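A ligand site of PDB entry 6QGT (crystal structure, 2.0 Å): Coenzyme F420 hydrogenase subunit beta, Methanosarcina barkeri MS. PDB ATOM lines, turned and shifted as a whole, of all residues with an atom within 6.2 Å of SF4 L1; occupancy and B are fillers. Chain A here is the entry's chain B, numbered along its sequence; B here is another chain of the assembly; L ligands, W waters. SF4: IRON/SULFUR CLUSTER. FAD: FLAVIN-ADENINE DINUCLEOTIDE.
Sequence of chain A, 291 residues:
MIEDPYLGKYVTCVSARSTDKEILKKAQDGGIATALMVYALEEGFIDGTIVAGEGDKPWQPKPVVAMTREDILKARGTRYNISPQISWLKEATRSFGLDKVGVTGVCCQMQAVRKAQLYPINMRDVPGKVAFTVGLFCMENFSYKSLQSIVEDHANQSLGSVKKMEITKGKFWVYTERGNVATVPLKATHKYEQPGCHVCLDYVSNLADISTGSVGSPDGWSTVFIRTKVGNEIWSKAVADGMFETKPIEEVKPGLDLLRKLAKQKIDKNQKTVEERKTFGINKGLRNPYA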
ATOM      1  N   VAL A 106      26.541  21.117   8.028  1.00  0.00           N
ATOM      2  CA  VAL A 106      25.600  20.025   7.844  1.00  0.00           C
ATOM      3  C   VAL A 106      24.279  20.570   7.299  1.00  0.00           C
ATOM      4  O   VAL A 106      24.148  21.772   7.019  1.00  0.00           O
ATOM      5  CB  VAL A 106      25.432  19.232   9.145  1.00  0.00           C
ATOM      6  CG1 VAL A 106      26.719  18.445   9.402  1.00  0.00           C
ATOM      7  CG2 VAL A 106      25.138  20.172  10.301  1.00  0.00           C
ATOM      8  N   CYS A 107      23.287  19.677   7.170  1.00  0.00           N
ATOM      9  CA  CYS A 107      22.072  19.999   6.420  1.00  0.00           C
ATOM     10  C   CYS A 107      21.367  21.234   6.969  1.00  0.00           C
ATOM     11  O   CYS A 107      20.972  22.115   6.199  1.00  0.00           O
ATOM     12  CB  CYS A 107      21.133  18.787   6.411  1.00  0.00           C
ATOM     13  SG  CYS A 107      22.037  17.237   6.031  1.00  0.00           S
ATOM     14  N   CYS A 108      21.205  21.319   8.298  1.00  0.00           N
ATOM     15  CA  CYS A 108      20.469  22.427   8.912  1.00  0.00           C
ATOM     16  C   CYS A 108      21.193  23.759   8.721  1.00  0.00           C
ATOM     17  O   CYS A 108      20.575  24.830   8.727  1.00  0.00           O
ATOM     18  CB  CYS A 108      20.272  22.167  10.403  1.00  0.00           C
ATOM     19  SG  CYS A 108      21.850  21.732  11.229  1.00  0.00           S
ATOM     20  N   GLN A 109      22.509  23.688   8.594  1.00  0.00           N
ATOM     21  CA  GLN A 109      23.296  24.885   8.379  1.00  0.00           C
ATOM     22  C   GLN A 109      23.168  25.343   6.931  1.00  0.00           C
ATOM     23  O   GLN A 109      23.104  26.548   6.651  1.00  0.00           O
ATOM     24  CB  GLN A 109      24.734  24.593   8.797  1.00  0.00           C
ATOM     25  CG  GLN A 109      24.856  24.511  10.304  1.00  0.00           C
ATOM     26  CD  GLN A 109      26.063  23.741  10.777  1.00  0.00           C
ATOM     27  OE1 GLN A 109      26.866  23.230   9.977  1.00  0.00           O
ATOM     28  NE2 GLN A 109      26.216  23.641  12.106  1.00  0.00           N
ATOM     29  N   LEU A 136      27.527  18.633   4.258  1.00  0.00           N
ATOM     30  CA  LEU A 136      27.829  17.263   4.659  1.00  0.00           C
ATOM     31  C   LEU A 136      26.538  16.494   4.875  1.00  0.00           C
ATOM     32  O   LEU A 136      25.529  17.066   5.300  1.00  0.00           O
ATOM     33  CB  LEU A 136      28.659  17.233   5.952  1.00  0.00           C
ATOM     34  CG  LEU A 136      29.787  18.241   6.154  1.00  0.00           C
ATOM     35  CD1 LEU A 136      30.600  17.869   7.389  1.00  0.00           C
ATOM     36  CD2 LEU A 136      30.668  18.360   4.943  1.00  0.00           C
ATOM     37  N   CYS A 138      24.327  14.226   7.206  1.00  0.00           N
ATOM     38  CA  CYS A 138      24.271  14.223   8.676  1.00  0.00           C
ATOM     39  C   CYS A 138      23.035  13.475   9.131  1.00  0.00           C
ATOM     40  O   CYS A 138      21.916  13.862   8.795  1.00  0.00           O
ATOM     41  CB  CYS A 138      24.263  15.672   9.220  1.00  0.00           C
ATOM     42  SG  CYS A 138      24.162  15.768  11.035  1.00  0.00           S
ATOM     43  N   MET A 139      23.237  12.402   9.920  1.00  0.00           N
ATOM     44  CA  MET A 139      22.152  11.648  10.507  1.00  0.00           C
ATOM     45  C   MET A 139      21.700  12.252  11.820  1.00  0.00           C
ATOM     46  O   MET A 139      20.485  12.343  12.070  1.00  0.00           O
ATOM     47  CB  MET A 139      22.571  10.181  10.748  1.00  0.00           C
ATOM     48  CG  MET A 139      21.454   9.287  11.247  1.00  0.00           C
ATOM     49  SD  MET A 139      20.038   9.180  10.100  1.00  0.00           S
ATOM     50  CE  MET A 139      20.691   8.009   8.926  1.00  0.00           C
ATOM     51  N   GLU A 140      22.645  12.678  12.659  1.00  0.00           N
ATOM     52  CA  GLU A 140      22.351  13.312  13.943  1.00  0.00           C
ATOM     53  C   GLU A 140      23.654  13.873  14.510  1.00  0.00           C
ATOM     54  O   GLU A 140      24.760  13.510  14.071  1.00  0.00           O
ATOM     55  CB  GLU A 140      21.679  12.343  14.932  1.00  0.00           C
ATOM     56  CG  GLU A 140      22.606  11.261  15.454  1.00  0.00           C
ATOM     57  CD  GLU A 140      22.479   9.942  14.695  1.00  0.00           C
ATOM     58  OE1 GLU A 140      21.329   9.438  14.601  1.00  0.00           O
ATOM     59  OE2 GLU A 140      23.510   9.419  14.202  1.00  0.00           O
ATOM     60  N   ASN A 141      23.517  14.763  15.509  1.00  0.00           N
ATOM     61  CA  ASN A 141      24.657  15.379  16.189  1.00  0.00           C
ATOM     62  C   ASN A 141      24.471  15.289  17.715  1.00  0.00           C
ATOM     63  O   ASN A 141      23.431  14.852  18.223  1.00  0.00           O
ATOM     64  CB  ASN A 141      24.851  16.849  15.755  1.00  0.00           C
ATOM     65  CG  ASN A 141      26.308  17.286  15.833  1.00  0.00           C
ATOM     66  OD1 ASN A 141      27.140  16.607  16.446  1.00  0.00           O
ATOM     67  ND2 ASN A 141      26.632  18.411  15.204  1.00  0.00           N
ATOM     68  N   GLN A 194      21.485  15.304  20.198  1.00  0.00           N
ATOM     69  CA  GLN A 194      20.899  16.617  20.414  1.00  0.00           C
ATOM     70  C   GLN A 194      19.418  16.550  20.076  1.00  0.00           C
ATOM     71  O   GLN A 194      19.063  16.128  18.962  1.00  0.00           O
ATOM     72  CB  GLN A 194      21.616  17.681  19.550  1.00  0.00           C
ATOM     73  CG  GLN A 194      20.817  18.981  19.437  1.00  0.00           C
ATOM     74  CD  GLN A 194      21.536  20.059  18.641  1.00  0.00           C
ATOM     75  OE1 GLN A 194      21.607  21.218  19.072  1.00  0.00           O
ATOM     76  NE2 GLN A 194      22.065  19.699  17.479  1.00  0.00           N
ATOM     77  N   GLY A 196      17.115  18.559  19.132  1.00  0.00           N
ATOM     78  CA  GLY A 196      16.661  19.279  17.959  1.00  0.00           C
ATOM     79  C   GLY A 196      16.936  18.581  16.631  1.00  0.00           C
ATOM     80  O   GLY A 196      16.395  18.991  15.612  1.00  0.00           O
ATOM     81  N   CYS A 197      17.767  17.532  16.634  1.00  0.00           N
ATOM     82  CA  CYS A 197      18.019  16.720  15.454  1.00  0.00           C
ATOM     83  C   CYS A 197      16.845  15.820  15.113  1.00  0.00           C
ATOM     84  O   CYS A 197      16.796  15.263  14.009  1.00  0.00           O
ATOM     85  CB  CYS A 197      19.264  15.869  15.670  1.00  0.00           C
ATOM     86  SG  CYS A 197      20.827  16.808  15.735  1.00  0.00           S
ATOM     87  N   HIS A 198      15.903  15.654  16.033  1.00  0.00           N
ATOM     88  CA  HIS A 198      14.853  14.645  15.889  1.00  0.00           C
ATOM     89  C   HIS A 198      13.681  15.122  15.051  1.00  0.00           C
ATOM     90  O   HIS A 198      12.682  14.411  14.911  1.00  0.00           O
ATOM     91  CB  HIS A 198      14.401  14.219  17.278  1.00  0.00           C
ATOM     92  CG  HIS A 198      15.481  13.513  18.050  1.00  0.00           C
ATOM     93  ND1 HIS A 198      15.439  13.368  19.425  1.00  0.00           N
ATOM     94  CD2 HIS A 198      16.595  12.882  17.632  1.00  0.00           C
ATOM     95  CE1 HIS A 198      16.504  12.685  19.820  1.00  0.00           C
ATOM     96  NE2 HIS A 198      17.224  12.382  18.755  1.00  0.00           N
ATOM     97  N   CYS A 200      14.553  16.905  12.128  1.00  0.00           N
ATOM     98  CA  CYS A 200      15.306  17.212  10.924  1.00  0.00           C
ATOM     99  C   CYS A 200      14.937  16.240   9.797  1.00  0.00           C
ATOM    100  O   CYS A 200      15.107  15.030   9.926  1.00  0.00           O
ATOM    101  CB  CYS A 200      16.802  17.121  11.206  1.00  0.00           C
ATOM    102  SG  CYS A 200      17.797  17.431   9.755  1.00  0.00           S
ATOM    103  N   LEU A 201      14.513  16.805   8.670  1.00  0.00           N
ATOM    104  CA  LEU A 201      13.979  16.041   7.542  1.00  0.00           C
ATOM    105  C   LEU A 201      14.890  16.151   6.317  1.00  0.00           C
ATOM    106  O   LEU A 201      14.430  16.275   5.177  1.00  0.00           O
ATOM    107  CB  LEU A 201      12.568  16.536   7.205  1.00  0.00           C
ATOM    108  CG  LEU A 201      11.683  16.743   8.453  1.00  0.00           C
ATOM    109  CD1 LEU A 201      10.414  17.525   8.125  1.00  0.00           C
ATOM    110  CD2 LEU A 201      11.337  15.417   9.155  1.00  0.00           C
ATOM    111  N   ASP A 202      16.203  16.127   6.558  1.00  0.00           N
ATOM    112  CA  ASP A 202      17.194  16.393   5.516  1.00  0.00           C
ATOM    113  C   ASP A 202      18.423  15.565   5.841  1.00  0.00           C
ATOM    114  O   ASP A 202      19.053  15.774   6.882  1.00  0.00           O
ATOM    115  CB  ASP A 202      17.522  17.894   5.457  1.00  0.00           C
ATOM    116  CG  ASP A 202      18.279  18.297   4.191  1.00  0.00           C
ATOM    117  OD1 ASP A 202      19.083  17.518   3.627  1.00  0.00           O
ATOM    118  OD2 ASP A 202      18.082  19.450   3.780  1.00  0.00           O
ATOM    119  N   LYS A 266      15.626   8.120   8.050  1.00  0.00           N
ATOM    120  CA  LYS A 266      15.758   9.379   8.785  1.00  0.00           C
ATOM    121  C   LYS A 266      14.493  10.209   8.664  1.00  0.00           C
ATOM    122  O   LYS A 266      13.869  10.553   9.684  1.00  0.00           O
ATOM    123  CB  LYS A 266      16.973  10.199   8.298  1.00  0.00           C
ATOM    124  CG  LYS A 266      17.115  11.489   9.152  1.00  0.00           C
ATOM    125  CD  LYS A 266      18.269  12.382   8.761  1.00  0.00           C
ATOM    126  CE  LYS A 266      18.485  13.560   9.772  1.00  0.00           C
ATOM    127  NZ  LYS A 266      19.596  14.457   9.315  1.00  0.00           N
ATOM    128  N   ASN A 270      11.791  10.984  11.697  1.00  0.00           N
ATOM    129  CA  ASN A 270      11.687  12.363  12.171  1.00  0.00           C
ATOM    130  C   ASN A 270      10.347  12.995  11.805  1.00  0.00           C
ATOM    131  O   ASN A 270       9.830  13.820  12.569  1.00  0.00           O
ATOM    132  CB  ASN A 270      12.850  13.185  11.615  1.00  0.00           C
ATOM    133  CG  ASN A 270      14.149  12.802  12.257  1.00  0.00           C
ATOM    134  OD1 ASN A 270      14.154  12.031  13.220  1.00  0.00           O
ATOM    135  ND2 ASN A 270      15.272  13.294  11.724  1.00  0.00           N
ATOM    136  N   MET B 189      18.908  23.606  17.104  1.00  0.00           N
ATOM    137  CA  MET B 189      19.953  22.676  16.644  1.00  0.00           C
ATOM    138  C   MET B 189      21.333  23.333  16.547  1.00  0.00           C
ATOM    139  O   MET B 189      22.218  22.780  15.881  1.00  0.00           O
ATOM    140  CB  MET B 189      19.600  21.997  15.303  1.00  0.00           C
ATOM    141  CG  MET B 189      18.943  22.871  14.266  1.00  0.00           C
ATOM    142  SD  MET B 189      20.046  24.196  13.719  1.00  0.00           S
ATOM    143  CE  MET B 189      18.921  25.148  12.670  1.00  0.00           C
ATOM    144  N   ARG B 229      14.559  27.654  12.737  1.00  0.00           N
ATOM    145  CA  ARG B 229      13.555  26.841  13.422  1.00  0.00           C
ATOM    146  C   ARG B 229      12.437  27.710  13.973  1.00  0.00           C
ATOM    147  O   ARG B 229      11.646  27.265  14.818  1.00  0.00           O
ATOM    148  CB  ARG B 229      14.220  25.984  14.509  1.00  0.00           C
ATOM    149  CG  ARG B 229      15.232  24.986  13.903  1.00  0.00           C
ATOM    150  CD  ARG B 229      14.478  23.793  13.299  1.00  0.00           C
ATOM    151  NE  ARG B 229      15.321  22.746  12.680  1.00  0.00           N
ATOM    152  CZ  ARG B 229      15.802  21.697  13.337  1.00  0.00           C
ATOM    153  NH1 ARG B 229      15.618  21.571  14.661  1.00  0.00           N
ATOM    154  NH2 ARG B 229      16.495  20.770  12.690  1.00  0.00           N
HETATM  155 FE1  SF4 L   1      21.559  19.595  11.896  1.00  0.00          FE
HETATM  156 FE2  SF4 L   1      19.714  17.728  11.099  1.00  0.00          FE
HETATM  157 FE3  SF4 L   1      20.876  17.568  13.631  1.00  0.00          FE
HETATM  158 FE4  SF4 L   1      22.413  16.933  11.502  1.00  0.00          FE
HETATM  159  S1  SF4 L   1      20.489  15.743  12.091  1.00  0.00           S
HETATM  160  S2  SF4 L   1      23.032  18.452  13.234  1.00  0.00           S
HETATM  161  S3  SF4 L   1      21.648  18.351   9.801  1.00  0.00           S
HETATM  162  S4  SF4 L   1      19.461  19.298  12.868  1.00  0.00           S
HETATM  163  PA  FAD L   2      37.209  16.831   5.137  1.00  0.00           P
HETATM  164  O1A FAD L   2      37.798  15.864   6.194  1.00  0.00           O
HETATM  165  O2A FAD L   2      38.150  17.165   4.085  1.00  0.00           O
HETATM  166  O5B FAD L   2      36.769  18.219   5.829  1.00  0.00           O
HETATM  167  C5B FAD L   2      35.918  18.263   6.950  1.00  0.00           C
HETATM  168  C4B FAD L   2      34.748  19.155   6.627  1.00  0.00           C
HETATM  169  O4B FAD L   2      33.773  18.852   7.513  1.00  0.00           O
HETATM  170  C3B FAD L   2      35.062  20.657   6.769  1.00  0.00           C
HETATM  171  O3B FAD L   2      34.305  21.308   5.848  1.00  0.00           O
HETATM  172  C2B FAD L   2      34.471  21.043   8.122  1.00  0.00           C
HETATM  173  O2B FAD L   2      34.168  22.526   8.084  1.00  0.00           O
HETATM  174  C1B FAD L   2      33.376  20.210   8.234  1.00  0.00           C
HETATM  175  N9A FAD L   2      33.062  19.750   9.529  1.00  0.00           N
HETATM  176  C8A FAD L   2      33.799  18.843  10.304  1.00  0.00           C
HETATM  177  N7A FAD L   2      33.061  18.705  11.566  1.00  0.00           N
HETATM  178  C5A FAD L   2      31.897  19.580  11.467  1.00  0.00           C
HETATM  179  C6A FAD L   2      30.855  19.878  12.332  1.00  0.00           C
HETATM  180  N6A FAD L   2      30.528  19.416  13.687  1.00  0.00           N
HETATM  181  N1A FAD L   2      29.851  20.758  11.994  1.00  0.00           N
HETATM  182  C2A FAD L   2      29.848  21.392  10.771  1.00  0.00           C
HETATM  183  N3A FAD L   2      30.874  21.102   9.882  1.00  0.00           N
HETATM  184  C4A FAD L   2      31.927  20.197  10.228  1.00  0.00           C
HETATM  185  N1  FAD L   2      28.301  11.326   6.453  1.00  0.00           N
HETATM  186  C2  FAD L   2      27.562  10.172   6.004  1.00  0.00           C
HETATM  187  O2  FAD L   2      27.845   9.643   4.948  1.00  0.00           O
HETATM  188  N3  FAD L   2      26.529   9.697   6.807  1.00  0.00           N
HETATM  189  C4  FAD L   2      26.197  10.310   8.063  1.00  0.00           C
HETATM  190  O4  FAD L   2      25.336   9.908   8.713  1.00  0.00           O
HETATM  191  C4X FAD L   2      26.974  11.485   8.540  1.00  0.00           C
HETATM  192  N5  FAD L   2      26.635  12.104   9.807  1.00  0.00           N
HETATM  193  C5X FAD L   2      27.458  13.265  10.122  1.00  0.00           C
HETATM  194  C6  FAD L   2      27.189  13.909  11.309  1.00  0.00           C
HETATM  195  C7  FAD L   2      27.963  15.016  11.649  1.00  0.00           C
HETATM  196  C7M FAD L   2      27.334  15.425  13.051  1.00  0.00           C
HETATM  197  C8  FAD L   2      29.021  15.485  10.788  1.00  0.00           C
HETATM  198  C8M FAD L   2      29.793  16.753  11.287  1.00  0.00           C
HETATM  199  C9  FAD L   2      29.312  14.889   9.620  1.00  0.00           C
HETATM  200  C9A FAD L   2      28.496  13.722   9.294  1.00  0.00           C
HETATM  201  N10 FAD L   2      28.787  13.071   8.059  1.00  0.00           N
HETATM  202  C10 FAD L   2      27.986  11.956   7.708  1.00  0.00           C
HETATM  203  C1' FAD L   2      29.848  13.540   7.134  1.00  0.00           C
HETATM  204  C2' FAD L   2      31.138  12.788   7.130  1.00  0.00           C
HETATM  205  O2' FAD L   2      31.380  12.434   8.435  1.00  0.00           O
HETATM  206  C3' FAD L   2      32.225  13.743   6.659  1.00  0.00           C
HETATM  207  O3' FAD L   2      32.088  14.888   7.430  1.00  0.00           O
HETATM  208  C4' FAD L   2      31.988  14.134   5.170  1.00  0.00           C
HETATM  209  O4' FAD L   2      32.070  12.970   4.387  1.00  0.00           O
HETATM  210  C5' FAD L   2      33.073  15.157   4.736  1.00  0.00           C
HETATM  211  O5' FAD L   2      34.250  14.437   4.597  1.00  0.00           O
HETATM  212  P   FAD L   2      35.415  14.952   3.684  1.00  0.00           P
HETATM  213  O1P FAD L   2      34.823  15.378   2.329  1.00  0.00           O
HETATM  214  O2P FAD L   2      36.584  14.062   3.586  1.00  0.00           O
HETATM  215  O3P FAD L   2      35.883  16.343   4.516  1.00  0.00           O
HETATM  216  O   HOH W   1      24.938  20.660  13.974  1.00  0.00           O
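The backbone carbonyl oxygen of Met 139 lies close to a sulfur (S1) of SF4 L1 (3.4 Å).
Residues that only touch SF4 L1: Val 106 (3.9 Å), Asn 141 (3.5 Å) and Met 189 of chain B (3.6 Å).
Hydrophobic or aromatic side chains within 4 Å of SF4 L1: Val 106 and Met 189 of chain B.
The side-chain amino group (NZ) of Lys 266 is in hydrogen-bond range of the backbone carbonyl oxygen (O) of Cys 138, 2.5 Å away.
SG of Cys 197 lies close to NE2 of Gln 194, at 3.6 Å.
The backbone carbonyl oxygen (O) of Asp 202 is in hydrogen-bond range of the side-chain amino group (NZ) of Lys 266, 2.8 Å away.
The side-chain sulfur (SG) of Cys 107 is in hydrogen-bond range of the backbone carbonyl oxygen (O) of Asp 202 (3.4 Å).
O of Leu 136 is in hydrogen-bond range of SG of Cys 107 (3.6 Å).
O of Asn 141 is in hydrogen-bond range of N of Gln 194, at 2.8 Å.
O of Met 189 of chain B lies within hydrogen-bond range of NE2 of Gln 194.
The side-chain amide oxygen (OE1) of Gln 109 sits at hydrogen-bond distance from the backbone NH (N) of Val 106 (2.9 Å).
Water W1 bridges S2 of SF4 L1 (3.0 Å) and ND2 of Asn 141 (3.1 Å).
FE4 of SF4 L1 is bound by SG of Cys 138 (2.2 Å).
The side-chain sulfur (SG) of Cys 197 binds an iron atom (FE3) of SF4 L1 (2.2 Å).
The backbone NH (N) of Cys 108 lies close to a sulfur (S3) of SF4 L1, 3.4 Å away.
The side-chain sulfur of Cys 108 binds an iron atom (FE1) of SF4 L1.
SG of Cys 200 is bound to FE2 of SF4 L1, 2.4 Å away.
The side-chain amino group (NZ) of Lys 266 sits close to a sulfur (S1) of SF4 L1, at 3.2 Å.
S4 of SF4 L1 sits close to NH2 of Arg 229 of chain B (3.3 Å).
The backbone NH (N) of Cys 107 lies close to a sulfur (S3) of SF4 L1, 3.4 Å away.
N of Glu 140 lies close to S1 of SF4 L1, at 3.8 Å.
N of Met 139 sits at hydrogen-bond distance from N5 of FAD L2 (3.4 Å).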
